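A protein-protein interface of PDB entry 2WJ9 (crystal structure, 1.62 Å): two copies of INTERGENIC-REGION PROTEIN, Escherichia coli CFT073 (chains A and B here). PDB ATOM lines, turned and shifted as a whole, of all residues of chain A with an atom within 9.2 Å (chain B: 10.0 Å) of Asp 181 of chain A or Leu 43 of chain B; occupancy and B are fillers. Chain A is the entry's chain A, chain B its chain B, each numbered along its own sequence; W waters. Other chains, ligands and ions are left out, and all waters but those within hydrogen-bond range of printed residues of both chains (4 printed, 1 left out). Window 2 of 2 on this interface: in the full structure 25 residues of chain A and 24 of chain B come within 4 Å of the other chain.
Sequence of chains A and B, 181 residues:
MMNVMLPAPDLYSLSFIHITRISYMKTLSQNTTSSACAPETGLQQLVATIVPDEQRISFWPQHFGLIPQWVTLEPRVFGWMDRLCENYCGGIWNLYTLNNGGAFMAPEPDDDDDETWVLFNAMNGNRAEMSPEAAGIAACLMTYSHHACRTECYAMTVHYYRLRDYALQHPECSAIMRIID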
ATOM      1  N   LEU A  84      -1.827  -7.969 -17.607  1.00  0.00           N
ATOM      2  CA  LEU A  84      -2.415  -7.981 -18.958  1.00  0.00           C
ATOM      3  C   LEU A  84      -3.822  -7.384 -19.029  1.00  0.00           C
ATOM      4  O   LEU A  84      -4.192  -6.790 -20.043  1.00  0.00           O
ATOM      5  CB  LEU A  84      -2.431  -9.409 -19.514  1.00  0.00           C
ATOM      6  CG  LEU A  84      -1.047 -10.010 -19.782  1.00  0.00           C
ATOM      7  CD1 LEU A  84      -1.121 -11.519 -19.967  1.00  0.00           C
ATOM      8  CD2 LEU A  84      -0.394  -9.349 -20.992  1.00  0.00           C
ATOM      9  N   ASN A 121      -0.407  -5.943 -23.617  1.00  0.00           N
ATOM     10  CA  ASN A 121       0.971  -6.273 -23.238  1.00  0.00           C
ATOM     11  C   ASN A 121       1.933  -5.129 -23.595  1.00  0.00           C
ATOM     12  O   ASN A 121       2.213  -4.875 -24.766  1.00  0.00           O
ATOM     13  CB  ASN A 121       1.414  -7.579 -23.911  1.00  0.00           C
ATOM     14  CG  ASN A 121       2.735  -8.107 -23.365  1.00  0.00           C
ATOM     15  OD1 ASN A 121       3.428  -7.421 -22.604  1.00  0.00           O
ATOM     16  ND2 ASN A 121       3.094  -9.328 -23.759  1.00  0.00           N
ATOM     17  N   ALA A 122       2.448  -4.456 -22.570  1.00  0.00           N
ATOM     18  CA  ALA A 122       3.361  -3.327 -22.764  1.00  0.00           C
ATOM     19  C   ALA A 122       4.725  -3.719 -23.356  1.00  0.00           C
ATOM     20  O   ALA A 122       5.421  -2.859 -23.911  1.00  0.00           O
ATOM     21  CB  ALA A 122       3.551  -2.584 -21.454  1.00  0.00           C
ATOM     22  N   MET A 123       5.104  -4.995 -23.229  1.00  0.00           N
ATOM     23  CA  MET A 123       6.376  -5.485 -23.775  1.00  0.00           C
ATOM     24  C   MET A 123       6.429  -5.331 -25.297  1.00  0.00           C
ATOM     25  O   MET A 123       7.474  -4.983 -25.853  1.00  0.00           O
ATOM     26  CB  MET A 123       6.608  -6.956 -23.413  1.00  0.00           C
ATOM     27  CG  MET A 123       6.932  -7.226 -21.947  1.00  0.00           C
ATOM     28  SD  MET A 123       7.456  -8.937 -21.672  1.00  0.00           S
ATOM     29  CE  MET A 123       9.075  -8.927 -22.444  1.00  0.00           C
ATOM     30  N   ASN A 124       5.299  -5.584 -25.967  1.00  0.00           N
ATOM     31  CA  ASN A 124       5.208  -5.484 -27.435  1.00  0.00           C
ATOM     32  C   ASN A 124       4.209  -4.439 -27.947  1.00  0.00           C
ATOM     33  O   ASN A 124       4.160  -4.165 -29.148  1.00  0.00           O
ATOM     34  CB  ASN A 124       4.919  -6.863 -28.065  1.00  0.00           C
ATOM     35  CG  ASN A 124       3.645  -7.519 -27.530  1.00  0.00           C
ATOM     36  OD1 ASN A 124       2.681  -6.844 -27.162  1.00  0.00           O
ATOM     37  ND2 ASN A 124       3.637  -8.850 -27.504  1.00  0.00           N
ATOM     38  N   GLY A 125       3.423  -3.860 -27.038  1.00  0.00           N
ATOM     39  CA  GLY A 125       2.469  -2.807 -27.386  1.00  0.00           C
ATOM     40  C   GLY A 125       1.174  -3.296 -28.015  1.00  0.00           C
ATOM     41  O   GLY A 125       0.402  -2.496 -28.536  1.00  0.00           O
ATOM     42  N   ASN A 126       0.924  -4.604 -27.954  1.00  0.00           N
ATOM     43  CA  ASN A 126      -0.245  -5.205 -28.609  1.00  0.00           C
ATOM     44  C   ASN A 126      -1.446  -5.312 -27.675  1.00  0.00           C
ATOM     45  O   ASN A 126      -1.299  -5.615 -26.490  1.00  0.00           O
ATOM     46  CB  ASN A 126       0.092  -6.602 -29.149  1.00  0.00           C
ATOM     47  CG  ASN A 126       1.116  -6.572 -30.268  1.00  0.00           C
ATOM     48  OD1 ASN A 126       1.346  -5.539 -30.891  1.00  0.00           O
ATOM     49  ND2 ASN A 126       1.724  -7.723 -30.541  1.00  0.00           N
ATOM     50  N   ARG A 127      -2.630  -5.067 -28.229  1.00  0.00           N
ATOM     51  CA  ARG A 127      -3.897  -5.223 -27.509  1.00  0.00           C
ATOM     52  C   ARG A 127      -4.723  -6.294 -28.216  1.00  0.00           C
ATOM     53  O   ARG A 127      -4.641  -6.414 -29.434  1.00  0.00           O
ATOM     54  CB  ARG A 127      -4.658  -3.899 -27.500  1.00  0.00           C
ATOM     55  CG  ARG A 127      -5.573  -3.691 -26.303  1.00  0.00           C
ATOM     56  CD  ARG A 127      -6.211  -2.307 -26.304  1.00  0.00           C
ATOM     57  NE  ARG A 127      -5.231  -1.222 -26.208  1.00  0.00           N
ATOM     58  CZ  ARG A 127      -4.657  -0.800 -25.079  1.00  0.00           C
ATOM     59  NH1 ARG A 127      -4.947  -1.366 -23.911  1.00  0.00           N
ATOM     60  NH2 ARG A 127      -3.778   0.197 -25.120  1.00  0.00           N
ATOM     61  N   ALA A 138      -2.884 -17.382 -22.133  1.00  0.00           N
ATOM     62  CA  ALA A 138      -1.897 -16.303 -22.351  1.00  0.00           C
ATOM     63  C   ALA A 138      -1.065 -15.966 -21.102  1.00  0.00           C
ATOM     64  O   ALA A 138       0.168 -15.869 -21.171  1.00  0.00           O
ATOM     65  CB  ALA A 138      -2.593 -15.048 -22.873  1.00  0.00           C
ATOM     66  N   LEU A 141       1.361 -18.913 -20.457  1.00  0.00           N
ATOM     67  CA  LEU A 141       2.473 -18.945 -21.428  1.00  0.00           C
ATOM     68  C   LEU A 141       3.571 -17.923 -21.089  1.00  0.00           C
ATOM     69  O   LEU A 141       4.762 -18.238 -21.180  1.00  0.00           O
ATOM     70  CB  LEU A 141       1.977 -18.731 -22.862  1.00  0.00           C
ATOM     71  CG  LEU A 141       1.237 -19.911 -23.501  1.00  0.00           C
ATOM     72  CD1 LEU A 141       0.518 -19.459 -24.757  1.00  0.00           C
ATOM     73  CD2 LEU A 141       2.171 -21.097 -23.784  1.00  0.00           C
ATOM     74  N   MET A 142       3.166 -16.719 -20.679  1.00  0.00           N
ATOM     75  CA  MET A 142       4.114 -15.689 -20.268  1.00  0.00           C
ATOM     76  C   MET A 142       4.841 -16.088 -18.984  1.00  0.00           C
ATOM     77  O   MET A 142       6.056 -15.930 -18.887  1.00  0.00           O
ATOM     78  CB  MET A 142       3.407 -14.351 -20.061  1.00  0.00           C
ATOM     79  CG  MET A 142       2.853 -13.727 -21.336  1.00  0.00           C
ATOM     80  SD  MET A 142       4.079 -13.257 -22.588  1.00  0.00           S
ATOM     81  CE  MET A 142       4.546 -14.807 -23.334  1.00  0.00           C
ATOM     82  N   HIS A 146       8.918 -16.897 -19.031  1.00  0.00           N
ATOM     83  CA  HIS A 146       9.734 -16.061 -18.159  1.00  0.00           C
ATOM     84  C   HIS A 146      10.450 -16.879 -17.075  1.00  0.00           C
ATOM     85  O   HIS A 146      11.622 -16.620 -16.777  1.00  0.00           O
ATOM     86  CB  HIS A 146       8.895 -14.926 -17.551  1.00  0.00           C
ATOM     87  CG  HIS A 146       8.777 -13.723 -18.440  1.00  0.00           C
ATOM     88  ND1 HIS A 146       9.344 -12.507 -18.124  1.00  0.00           N
ATOM     89  CD2 HIS A 146       8.176 -13.556 -19.642  1.00  0.00           C
ATOM     90  CE1 HIS A 146       9.081 -11.637 -19.084  1.00  0.00           C
ATOM     91  NE2 HIS A 146       8.383 -12.252 -20.023  1.00  0.00           N
ATOM     92  N   TYR A 160       6.108 -24.611 -21.573  1.00  0.00           N
ATOM     93  CA  TYR A 160       5.780 -23.592 -22.581  1.00  0.00           C
ATOM     94  C   TYR A 160       5.358 -24.194 -23.911  1.00  0.00           C
ATOM     95  O   TYR A 160       4.300 -23.847 -24.433  1.00  0.00           O
ATOM     96  CB  TYR A 160       6.928 -22.607 -22.830  1.00  0.00           C
ATOM     97  CG  TYR A 160       6.675 -21.756 -24.066  1.00  0.00           C
ATOM     98  CD1 TYR A 160       5.891 -20.601 -24.001  1.00  0.00           C
ATOM     99  CD2 TYR A 160       7.171 -22.138 -25.314  1.00  0.00           C
ATOM    100  CE1 TYR A 160       5.631 -19.839 -25.140  1.00  0.00           C
ATOM    101  CE2 TYR A 160       6.911 -21.389 -26.457  1.00  0.00           C
ATOM    102  CZ  TYR A 160       6.149 -20.236 -26.367  1.00  0.00           C
ATOM    103  OH  TYR A 160       5.897 -19.503 -27.511  1.00  0.00           O
ATOM    104  N   ARG A 164       1.693 -24.133 -25.537  1.00  0.00           N
ATOM    105  CA  ARG A 164       1.679 -23.388 -26.790  1.00  0.00           C
ATOM    106  C   ARG A 164       1.018 -24.185 -27.918  1.00  0.00           C
ATOM    107  O   ARG A 164       0.236 -23.631 -28.701  1.00  0.00           O
ATOM    108  CB  ARG A 164       3.089 -22.982 -27.193  1.00  0.00           C
ATOM    109  CG  ARG A 164       3.120 -22.000 -28.349  1.00  0.00           C
ATOM    110  CD  ARG A 164       4.283 -22.215 -29.238  1.00  0.00           C
ATOM    111  NE  ARG A 164       4.305 -23.555 -29.841  1.00  0.00           N
ATOM    112  CZ  ARG A 164       5.256 -23.969 -30.661  1.00  0.00           C
ATOM    113  NH1 ARG A 164       6.238 -23.148 -30.990  1.00  0.00           N
ATOM    114  NH2 ARG A 164       5.236 -25.202 -31.152  1.00  0.00           N
ATOM    115  N   ALA A 167      -2.610 -23.889 -27.583  1.00  0.00           N
ATOM    116  CA  ALA A 167      -3.002 -22.578 -28.121  1.00  0.00           C
ATOM    117  C   ALA A 167      -3.079 -22.562 -29.653  1.00  0.00           C
ATOM    118  O   ALA A 167      -3.980 -21.953 -30.225  1.00  0.00           O
ATOM    119  CB  ALA A 167      -2.046 -21.504 -27.652  1.00  0.00           C
ATOM    120  N   LEU A 168      -2.145 -23.240 -30.317  1.00  0.00           N
ATOM    121  CA  LEU A 168      -2.138 -23.288 -31.787  1.00  0.00           C
ATOM    122  C   LEU A 168      -3.390 -23.917 -32.395  1.00  0.00           C
ATOM    123  O   LEU A 168      -3.813 -23.525 -33.482  1.00  0.00           O
ATOM    124  CB  LEU A 168      -0.901 -24.029 -32.306  1.00  0.00           C
ATOM    125  CG  LEU A 168       0.440 -23.317 -32.154  1.00  0.00           C
ATOM    126  CD1 LEU A 168       1.536 -24.234 -32.693  1.00  0.00           C
ATOM    127  CD2 LEU A 168       0.472 -21.966 -32.867  1.00  0.00           C
ATOM    128  N   CYS A 173      -6.457 -18.847 -31.197  1.00  0.00           N
ATOM    129  CA  CYS A 173      -5.015 -18.827 -31.440  1.00  0.00           C
ATOM    130  C   CYS A 173      -4.507 -17.429 -31.805  1.00  0.00           C
ATOM    131  O   CYS A 173      -3.489 -16.992 -31.278  1.00  0.00           O
ATOM    132  CB  CYS A 173      -4.643 -19.822 -32.551  1.00  0.00           C
ATOM    133  SG  CYS A 173      -2.853 -19.898 -32.952  1.00  0.00           S
ATOM    134  N   SER A 174      -5.225 -16.723 -32.680  1.00  0.00           N
ATOM    135  CA  SER A 174      -4.739 -15.429 -33.203  1.00  0.00           C
ATOM    136  C   SER A 174      -4.544 -14.412 -32.086  1.00  0.00           C
ATOM    137  O   SER A 174      -3.522 -13.727 -32.036  1.00  0.00           O
ATOM    138  CB  SER A 174      -5.684 -14.859 -34.268  1.00  0.00           C
ATOM    139  OG  SER A 174      -5.646 -15.634 -35.455  1.00  0.00           O
ATOM    140  N   ALA A 175      -5.526 -14.327 -31.191  1.00  0.00           N
ATOM    141  CA  ALA A 175      -5.471 -13.397 -30.063  1.00  0.00           C
ATOM    142  C   ALA A 175      -4.382 -13.813 -29.077  1.00  0.00           C
ATOM    143  O   ALA A 175      -3.639 -12.963 -28.569  1.00  0.00           O
ATOM    144  CB  ALA A 175      -6.830 -13.314 -29.358  1.00  0.00           C
ATOM    145  N   ILE A 176      -4.285 -15.117 -28.815  1.00  0.00           N
ATOM    146  CA  ILE A 176      -3.291 -15.640 -27.866  1.00  0.00           C
ATOM    147  C   ILE A 176      -1.877 -15.341 -28.377  1.00  0.00           C
ATOM    148  O   ILE A 176      -1.064 -14.781 -27.648  1.00  0.00           O
ATOM    149  CB  ILE A 176      -3.459 -17.160 -27.588  1.00  0.00           C
ATOM    150  CG1 ILE A 176      -4.824 -17.451 -26.957  1.00  0.00           C
ATOM    151  CG2 ILE A 176      -2.364 -17.666 -26.647  1.00  0.00           C
ATOM    152  CD1 ILE A 176      -5.240 -18.909 -26.995  1.00  0.00           C
ATOM    153  N   MET A 177      -1.596 -15.689 -29.633  1.00  0.00           N
ATOM    154  CA  MET A 177      -0.255 -15.477 -30.210  1.00  0.00           C
ATOM    155  C   MET A 177       0.082 -13.997 -30.355  1.00  0.00           C
ATOM    156  O   MET A 177       1.246 -13.601 -30.273  1.00  0.00           O
ATOM    157  CB  MET A 177      -0.121 -16.168 -31.567  1.00  0.00           C
ATOM    158  CG  MET A 177      -0.236 -17.684 -31.498  1.00  0.00           C
ATOM    159  SD  MET A 177       1.029 -18.479 -30.474  1.00  0.00           S
ATOM    160  CE  MET A 177       0.064 -19.801 -29.747  1.00  0.00           C
ATOM    161  N   ARG A 178      -0.934 -13.179 -30.582  1.00  0.00           N
ATOM    162  CA  ARG A 178      -0.712 -11.747 -30.708  1.00  0.00           C
ATOM    163  C   ARG A 178      -0.229 -11.142 -29.389  1.00  0.00           C
ATOM    164  O   ARG A 178       0.745 -10.379 -29.358  1.00  0.00           O
ATOM    165  CB  ARG A 178      -1.981 -11.051 -31.172  1.00  0.00           C
ATOM    166  CG  ARG A 178      -1.888  -9.552 -31.094  1.00  0.00           C
ATOM    167  CD  ARG A 178      -2.891  -8.906 -31.986  1.00  0.00           C
ATOM    168  NE  ARG A 178      -2.865  -7.457 -31.844  1.00  0.00           N
ATOM    169  CZ  ARG A 178      -1.931  -6.652 -32.345  1.00  0.00           C
ATOM    170  NH1 ARG A 178      -0.907  -7.135 -33.038  1.00  0.00           N
ATOM    171  NH2 ARG A 178      -2.034  -5.343 -32.147  1.00  0.00           N
ATOM    172  N   ILE A 179      -0.906 -11.495 -28.300  1.00  0.00           N
ATOM    173  CA  ILE A 179      -0.608 -10.897 -27.005  1.00  0.00           C
ATOM    174  C   ILE A 179       0.781 -11.343 -26.487  1.00  0.00           C
ATOM    175  O   ILE A 179       1.422 -10.612 -25.730  1.00  0.00           O
ATOM    176  CB  ILE A 179      -1.771 -11.166 -25.991  1.00  0.00           C
ATOM    177  CG1 ILE A 179      -1.888 -10.025 -24.975  1.00  0.00           C
ATOM    178  CG2 ILE A 179      -1.617 -12.507 -25.304  1.00  0.00           C
ATOM    179  CD1 ILE A 179      -2.171  -8.671 -25.592  1.00  0.00           C
ATOM    180  N   ILE A 180       1.259 -12.507 -26.936  1.00  0.00           N
ATOM    181  CA  ILE A 180       2.599 -13.001 -26.567  1.00  0.00           C
ATOM    182  C   ILE A 180       3.687 -12.823 -27.655  1.00  0.00           C
ATOM    183  O   ILE A 180       4.781 -13.384 -27.537  1.00  0.00           O
ATOM    184  CB  ILE A 180       2.559 -14.491 -26.108  1.00  0.00           C
ATOM    185  CG1 ILE A 180       2.325 -15.461 -27.276  1.00  0.00           C
ATOM    186  CG2 ILE A 180       1.486 -14.691 -25.039  1.00  0.00           C
ATOM    187  CD1 ILE A 180       2.442 -16.904 -26.874  1.00  0.00           C
ATOM    188  N   ASP A 181       3.408 -12.032 -28.692  1.00  0.00           N
ATOM    189  CA  ASP A 181       4.361 -11.857 -29.801  1.00  0.00           C
ATOM    190  C   ASP A 181       5.671 -11.221 -29.329  1.00  0.00           C
ATOM    191  O   ASP A 181       5.670 -10.424 -28.389  1.00  0.00           O
ATOM    192  CB  ASP A 181       3.761 -10.995 -30.918  1.00  0.00           C
ATOM    193  CG  ASP A 181       4.573 -11.059 -32.215  1.00  0.00           C
ATOM    194  OD1 ASP A 181       4.841 -12.179 -32.702  1.00  0.00           O
ATOM    195  OD2 ASP A 181       4.930  -9.990 -32.765  1.00  0.00           O
ATOM    196  OXT ASP A 181       6.748 -11.494 -29.879  1.00  0.00           O
ATOM    197  N   ALA B  38      13.745 -18.896 -24.230  1.00  0.00           N
ATOM    198  CA  ALA B  38      13.339 -18.689 -25.627  1.00  0.00           C
ATOM    199  C   ALA B  38      13.748 -17.295 -26.151  1.00  0.00           C
ATOM    200  O   ALA B  38      13.464 -16.293 -25.501  1.00  0.00           O
ATOM    201  CB  ALA B  38      11.836 -18.876 -25.752  1.00  0.00           C
ATOM    202  N   PRO B  39      14.436 -17.226 -27.314  1.00  0.00           N
ATOM    203  CA  PRO B  39      14.684 -15.946 -27.999  1.00  0.00           C
ATOM    204  C   PRO B  39      13.408 -15.134 -28.280  1.00  0.00           C
ATOM    205  O   PRO B  39      13.403 -13.909 -28.127  1.00  0.00           O
ATOM    206  CB  PRO B  39      15.335 -16.386 -29.318  1.00  0.00           C
ATOM    207  CG  PRO B  39      15.998 -17.654 -28.993  1.00  0.00           C
ATOM    208  CD  PRO B  39      15.082 -18.341 -28.030  1.00  0.00           C
ATOM    209  N   GLU B  40      12.350 -15.828 -28.705  1.00  0.00           N
ATOM    210  CA  GLU B  40      11.029 -15.225 -28.902  1.00  0.00           C
ATOM    211  C   GLU B  40       9.920 -16.205 -28.514  1.00  0.00           C
ATOM    212  O   GLU B  40      10.112 -17.421 -28.561  1.00  0.00           O
ATOM    213  CB  GLU B  40      10.808 -14.827 -30.366  1.00  0.00           C
ATOM    214  CG  GLU B  40      11.893 -13.955 -30.984  1.00  0.00           C
ATOM    215  CD  GLU B  40      11.486 -13.344 -32.328  1.00  0.00           C
ATOM    216  OE1 GLU B  40      10.314 -13.497 -32.760  1.00  0.00           O
ATOM    217  OE2 GLU B  40      12.348 -12.687 -32.954  1.00  0.00           O
ATOM    218  N   THR B  41       8.763 -15.660 -28.142  1.00  0.00           N
ATOM    219  CA  THR B  41       7.553 -16.462 -27.952  1.00  0.00           C
ATOM    220  C   THR B  41       6.581 -16.137 -29.095  1.00  0.00           C
ATOM    221  O   THR B  41       6.828 -15.229 -29.889  1.00  0.00           O
ATOM    222  CB  THR B  41       6.901 -16.203 -26.575  1.00  0.00           C
ATOM    223  OG1 THR B  41       6.735 -14.796 -26.367  1.00  0.00           O
ATOM    224  CG2 THR B  41       7.767 -16.783 -25.456  1.00  0.00           C
ATOM    225  N   GLY B  42       5.491 -16.890 -29.192  1.00  0.00           N
ATOM    226  CA  GLY B  42       4.534 -16.714 -30.288  1.00  0.00           C
ATOM    227  C   GLY B  42       5.043 -17.209 -31.642  1.00  0.00           C
ATOM    228  O   GLY B  42       5.826 -18.169 -31.716  1.00  0.00           O
ATOM    229  N   LEU B  43       4.573 -16.564 -32.711  1.00  0.00           N
ATOM    230  CA  LEU B  43       4.926 -16.938 -34.092  1.00  0.00           C
ATOM    231  C   LEU B  43       6.272 -16.324 -34.507  1.00  0.00           C
ATOM    232  O   LEU B  43       6.502 -15.142 -34.270  1.00  0.00           O
ATOM    233  CB  LEU B  43       3.826 -16.480 -35.059  1.00  0.00           C
ATOM    234  CG  LEU B  43       2.415 -17.051 -34.837  1.00  0.00           C
ATOM    235  CD1 LEU B  43       1.392 -16.368 -35.735  1.00  0.00           C
ATOM    236  CD2 LEU B  43       2.396 -18.571 -35.056  1.00  0.00           C
ATOM    237  N   GLN B  44       7.134 -17.113 -35.154  1.00  0.00           N
ATOM    238  CA  GLN B  44       8.493 -16.669 -35.516  1.00  0.00           C
ATOM    239  C   GLN B  44       9.027 -17.360 -36.776  1.00  0.00           C
ATOM    240  O   GLN B  44       8.933 -18.582 -36.895  1.00  0.00           O
ATOM    241  CB  GLN B  44       9.465 -16.935 -34.359  1.00  0.00           C
ATOM    242  CG  GLN B  44      10.956 -16.776 -34.729  1.00  0.00           C
ATOM    243  CD  GLN B  44      11.908 -17.201 -33.622  1.00  0.00           C
ATOM    244  OE1 GLN B  44      11.604 -18.086 -32.816  1.00  0.00           O
ATOM    245  NE2 GLN B  44      13.088 -16.585 -33.599  1.00  0.00           N
ATOM    246  N   GLN B  45       9.624 -16.576 -37.681  1.00  0.00           N
ATOM    247  CA  GLN B  45      10.296 -17.132 -38.866  1.00  0.00           C
ATOM    248  C   GLN B  45      11.606 -17.784 -38.447  1.00  0.00           C
ATOM    249  O   GLN B  45      12.509 -17.107 -37.946  1.00  0.00           O
ATOM    250  CB  GLN B  45      10.595 -16.054 -39.917  1.00  0.00           C
ATOM    251  CG  GLN B  45      11.451 -16.543 -41.106  1.00  0.00           C
ATOM    252  CD  GLN B  45      10.799 -17.674 -41.885  1.00  0.00           C
ATOM    253  OE1 GLN B  45      11.378 -18.748 -42.061  1.00  0.00           O
ATOM    254  NE2 GLN B  45       9.583 -17.446 -42.327  1.00  0.00           N
ATOM    255  N   LEU B  46      11.713 -19.086 -38.690  1.00  0.00           N
ATOM    256  CA  LEU B  46      12.881 -19.858 -38.270  1.00  0.00           C
ATOM    257  C   LEU B  46      13.895 -19.984 -39.418  1.00  0.00           C
ATOM    258  O   LEU B  46      13.522 -20.147 -40.593  1.00  0.00           O
ATOM    259  CB  LEU B  46      12.454 -21.226 -37.721  1.00  0.00           C
ATOM    260  CG  LEU B  46      11.504 -21.151 -36.517  1.00  0.00           C
ATOM    261  CD1 LEU B  46      10.992 -22.532 -36.127  1.00  0.00           C
ATOM    262  CD2 LEU B  46      12.151 -20.467 -35.297  1.00  0.00           C
ATOM    263  N   ASN B  99      17.667 -20.114 -35.027  1.00  0.00           N
ATOM    264  CA  ASN B  99      17.459 -18.853 -34.271  1.00  0.00           C
ATOM    265  C   ASN B  99      16.428 -18.943 -33.127  1.00  0.00           C
ATOM    266  O   ASN B  99      16.085 -17.911 -32.506  1.00  0.00           O
ATOM    267  CB  ASN B  99      17.116 -17.699 -35.222  1.00  0.00           C
ATOM    268  CG  ASN B  99      15.852 -17.947 -36.033  1.00  0.00           C
ATOM    269  OD1 ASN B  99      15.430 -19.086 -36.209  1.00  0.00           O
ATOM    270  ND2 ASN B  99      15.251 -16.878 -36.542  1.00  0.00           N
ATOM    271  N   ASN B 100      15.913 -20.148 -32.876  1.00  0.00           N
ATOM    272  CA  ASN B 100      15.123 -20.432 -31.672  1.00  0.00           C
ATOM    273  C   ASN B 100      15.921 -21.189 -30.594  1.00  0.00           C
ATOM    274  O   ASN B 100      15.357 -21.612 -29.589  1.00  0.00           O
ATOM    275  CB  ASN B 100      13.842 -21.191 -32.022  1.00  0.00           C
ATOM    276  CG  ASN B 100      14.111 -22.579 -32.608  1.00  0.00           C
ATOM    277  OD1 ASN B 100      15.264 -22.959 -32.857  1.00  0.00           O
ATOM    278  ND2 ASN B 100      13.038 -23.339 -32.821  1.00  0.00           N
ATOM    279  N   ASP B 165       9.731 -27.570 -34.769  1.00  0.00           N
ATOM    280  CA  ASP B 165       9.156 -26.315 -35.291  1.00  0.00           C
ATOM    281  C   ASP B 165       9.741 -25.917 -36.654  1.00  0.00           C
ATOM    282  O   ASP B 165       9.009 -25.484 -37.538  1.00  0.00           O
ATOM    283  CB  ASP B 165       9.358 -25.153 -34.307  1.00  0.00           C
ATOM    284  CG  ASP B 165       8.317 -25.112 -33.206  1.00  0.00           C
ATOM    285  OD1 ASP B 165       7.429 -25.997 -33.141  1.00  0.00           O
ATOM    286  OD2 ASP B 165       8.381 -24.156 -32.396  1.00  0.00           O
ATOM    287  N   GLN B 169       7.742 -25.763 -40.500  1.00  0.00           N
ATOM    288  CA  GLN B 169       7.782 -24.628 -41.429  1.00  0.00           C
ATOM    289  C   GLN B 169       8.457 -24.964 -42.768  1.00  0.00           C
ATOM    290  O   GLN B 169       8.474 -24.133 -43.677  1.00  0.00           O
ATOM    291  CB  GLN B 169       8.513 -23.437 -40.795  1.00  0.00           C
ATOM    292  CG  GLN B 169       7.812 -22.841 -39.564  1.00  0.00           C
ATOM    293  CD  GLN B 169       8.478 -21.581 -39.034  1.00  0.00           C
ATOM    294  OE1 GLN B 169       9.478 -21.098 -39.577  1.00  0.00           O
ATOM    295  NE2 GLN B 169       7.904 -21.026 -37.969  1.00  0.00           N
HETATM  296  O   HOH W   1       8.881 -12.804 -28.476  1.00  0.00           O
HETATM  297  O   HOH W   2       6.518 -20.225 -30.052  1.00  0.00           O
HETATM  298  O   HOH W   3       2.926 -14.112 -32.396  1.00  0.00           O
HETATM  299  O   HOH W   4       6.238 -12.644 -35.424  1.00  0.00           O
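Printed residues of chain B within 4 Å of Tyr 160 of chain A: Thr 41 and Gly 42. Of the printed residues of chain B, Arg 164 of chain A touches Asp 165 (2.8 Å). Of the printed residues of chain B, Met 177 of chain A touches Gly 42. Printed residues of chain B within 4 Å of Ile 180 of chain A: Thr 41 (2.7 Å) and Gly 42 (3.8 Å). Printed residues of chain B within 4 Å of Asp 181 of chain A: Thr 41 and Leu 43. Printed residues of chain A within 4 Å of Thr 41 of chain B: Met 142, Tyr 160, Ile 180 and Asp 181. Gly 42 of chain B touches just these residues of chain A: Tyr 160 (3.1 Å), Met 177 (3.9 Å) and Ile 180 (3.8 Å). Of chain A, only Asp 181 comes within 4 Å of Leu 43 of chain B. Printed residues of chain A within 4 Å of Asp 165 of chain B: Arg 164 (2.8 Å). The nearest residue of chain B that does not touch Asp 181 of chain A is Gly 42 of chain B (4.9 Å). The nearest residue of chain A that does not touch Leu 43 of chain B is Met 177 of chain A (4.2 Å).
No position is printed for both chains. Of the 9 pairs that touch across the chains among the printed residues, none has its exchanged pair printed and touching as well.
Water W2 lies within hydrogen-bond range of OH of Tyr 160 of chain A (2.7 Å), O of Gly 42 of chain B (2.7 Å) and NH1 of Arg 164 of chain A (3.1 Å). Water W3 lies within hydrogen-bond range of the side-chain carboxylate of Asp 181 of chain A, the backbone carbonyl oxygen of Met 177 of chain A and the backbone NH of Leu 43 of chain B. Water W4 lies within hydrogen-bond range of O of Leu 43 of chain B (2.8 Å) and OD1 of Asp 181 of chain A (3.1 Å). Water W1 bridges the chain-end carboxylate of Asp 181 of chain A and the backbone NH of Thr 41 of chain B.
N of Gly 42 of chain B lies within hydrogen-bond range of OH of Tyr 160 of chain A, at 3.1 Å. The side-chain carboxylate (OD2) of Asp 165 of chain B is in salt-bridge range of the guanidinium group (NH1) of Arg 164 of chain A (2.8 Å). O of Ile 180 of chain A is in hydrogen-bond range of OG1 of Thr 41 of chain B (2.7 Å).
Thr 41 of chain B touches Met 142 of chain A (OG1 to CE, 3.7 Å). Thr 41 of chain B touches Tyr 160 of chain A. Met 177 of chain A touches Gly 42 of chain B (SD to CA, 3.9 Å). Ile 180 of chain A touches Gly 42 of chain B (CD1 to N, 3.8 Å). Asp 181 of chain A touches Thr 41 of chain B (OXT to O, 3.7 Å). OD1 of Asp 181 of chain A touches O of Leu 43 of chain B, at 3.7 Å.
Of the 25 printed residues of chain A, 6 touch a printed residue of chain B. Printed residues of chain A that touch a printed residue of chain B: Met 142, Tyr 160, Arg 164, Met 177, Ile 180 and Asp 181. Hydrophobic or aromatic side chains of chain A within 4 Å of the printed part of chain B: Met 142, Tyr 160, Met 177 and Ile 180. Along chain A the printed residues that touch a printed residue of chain B span positions 142 to 181. Of the 13 printed residues of chain B, 4 touch a printed residue of chain A.
ND2 of Asn 124 of chain A sits at hydrogen-bond distance from O of Asp 181 of chain A (2.7 Å).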
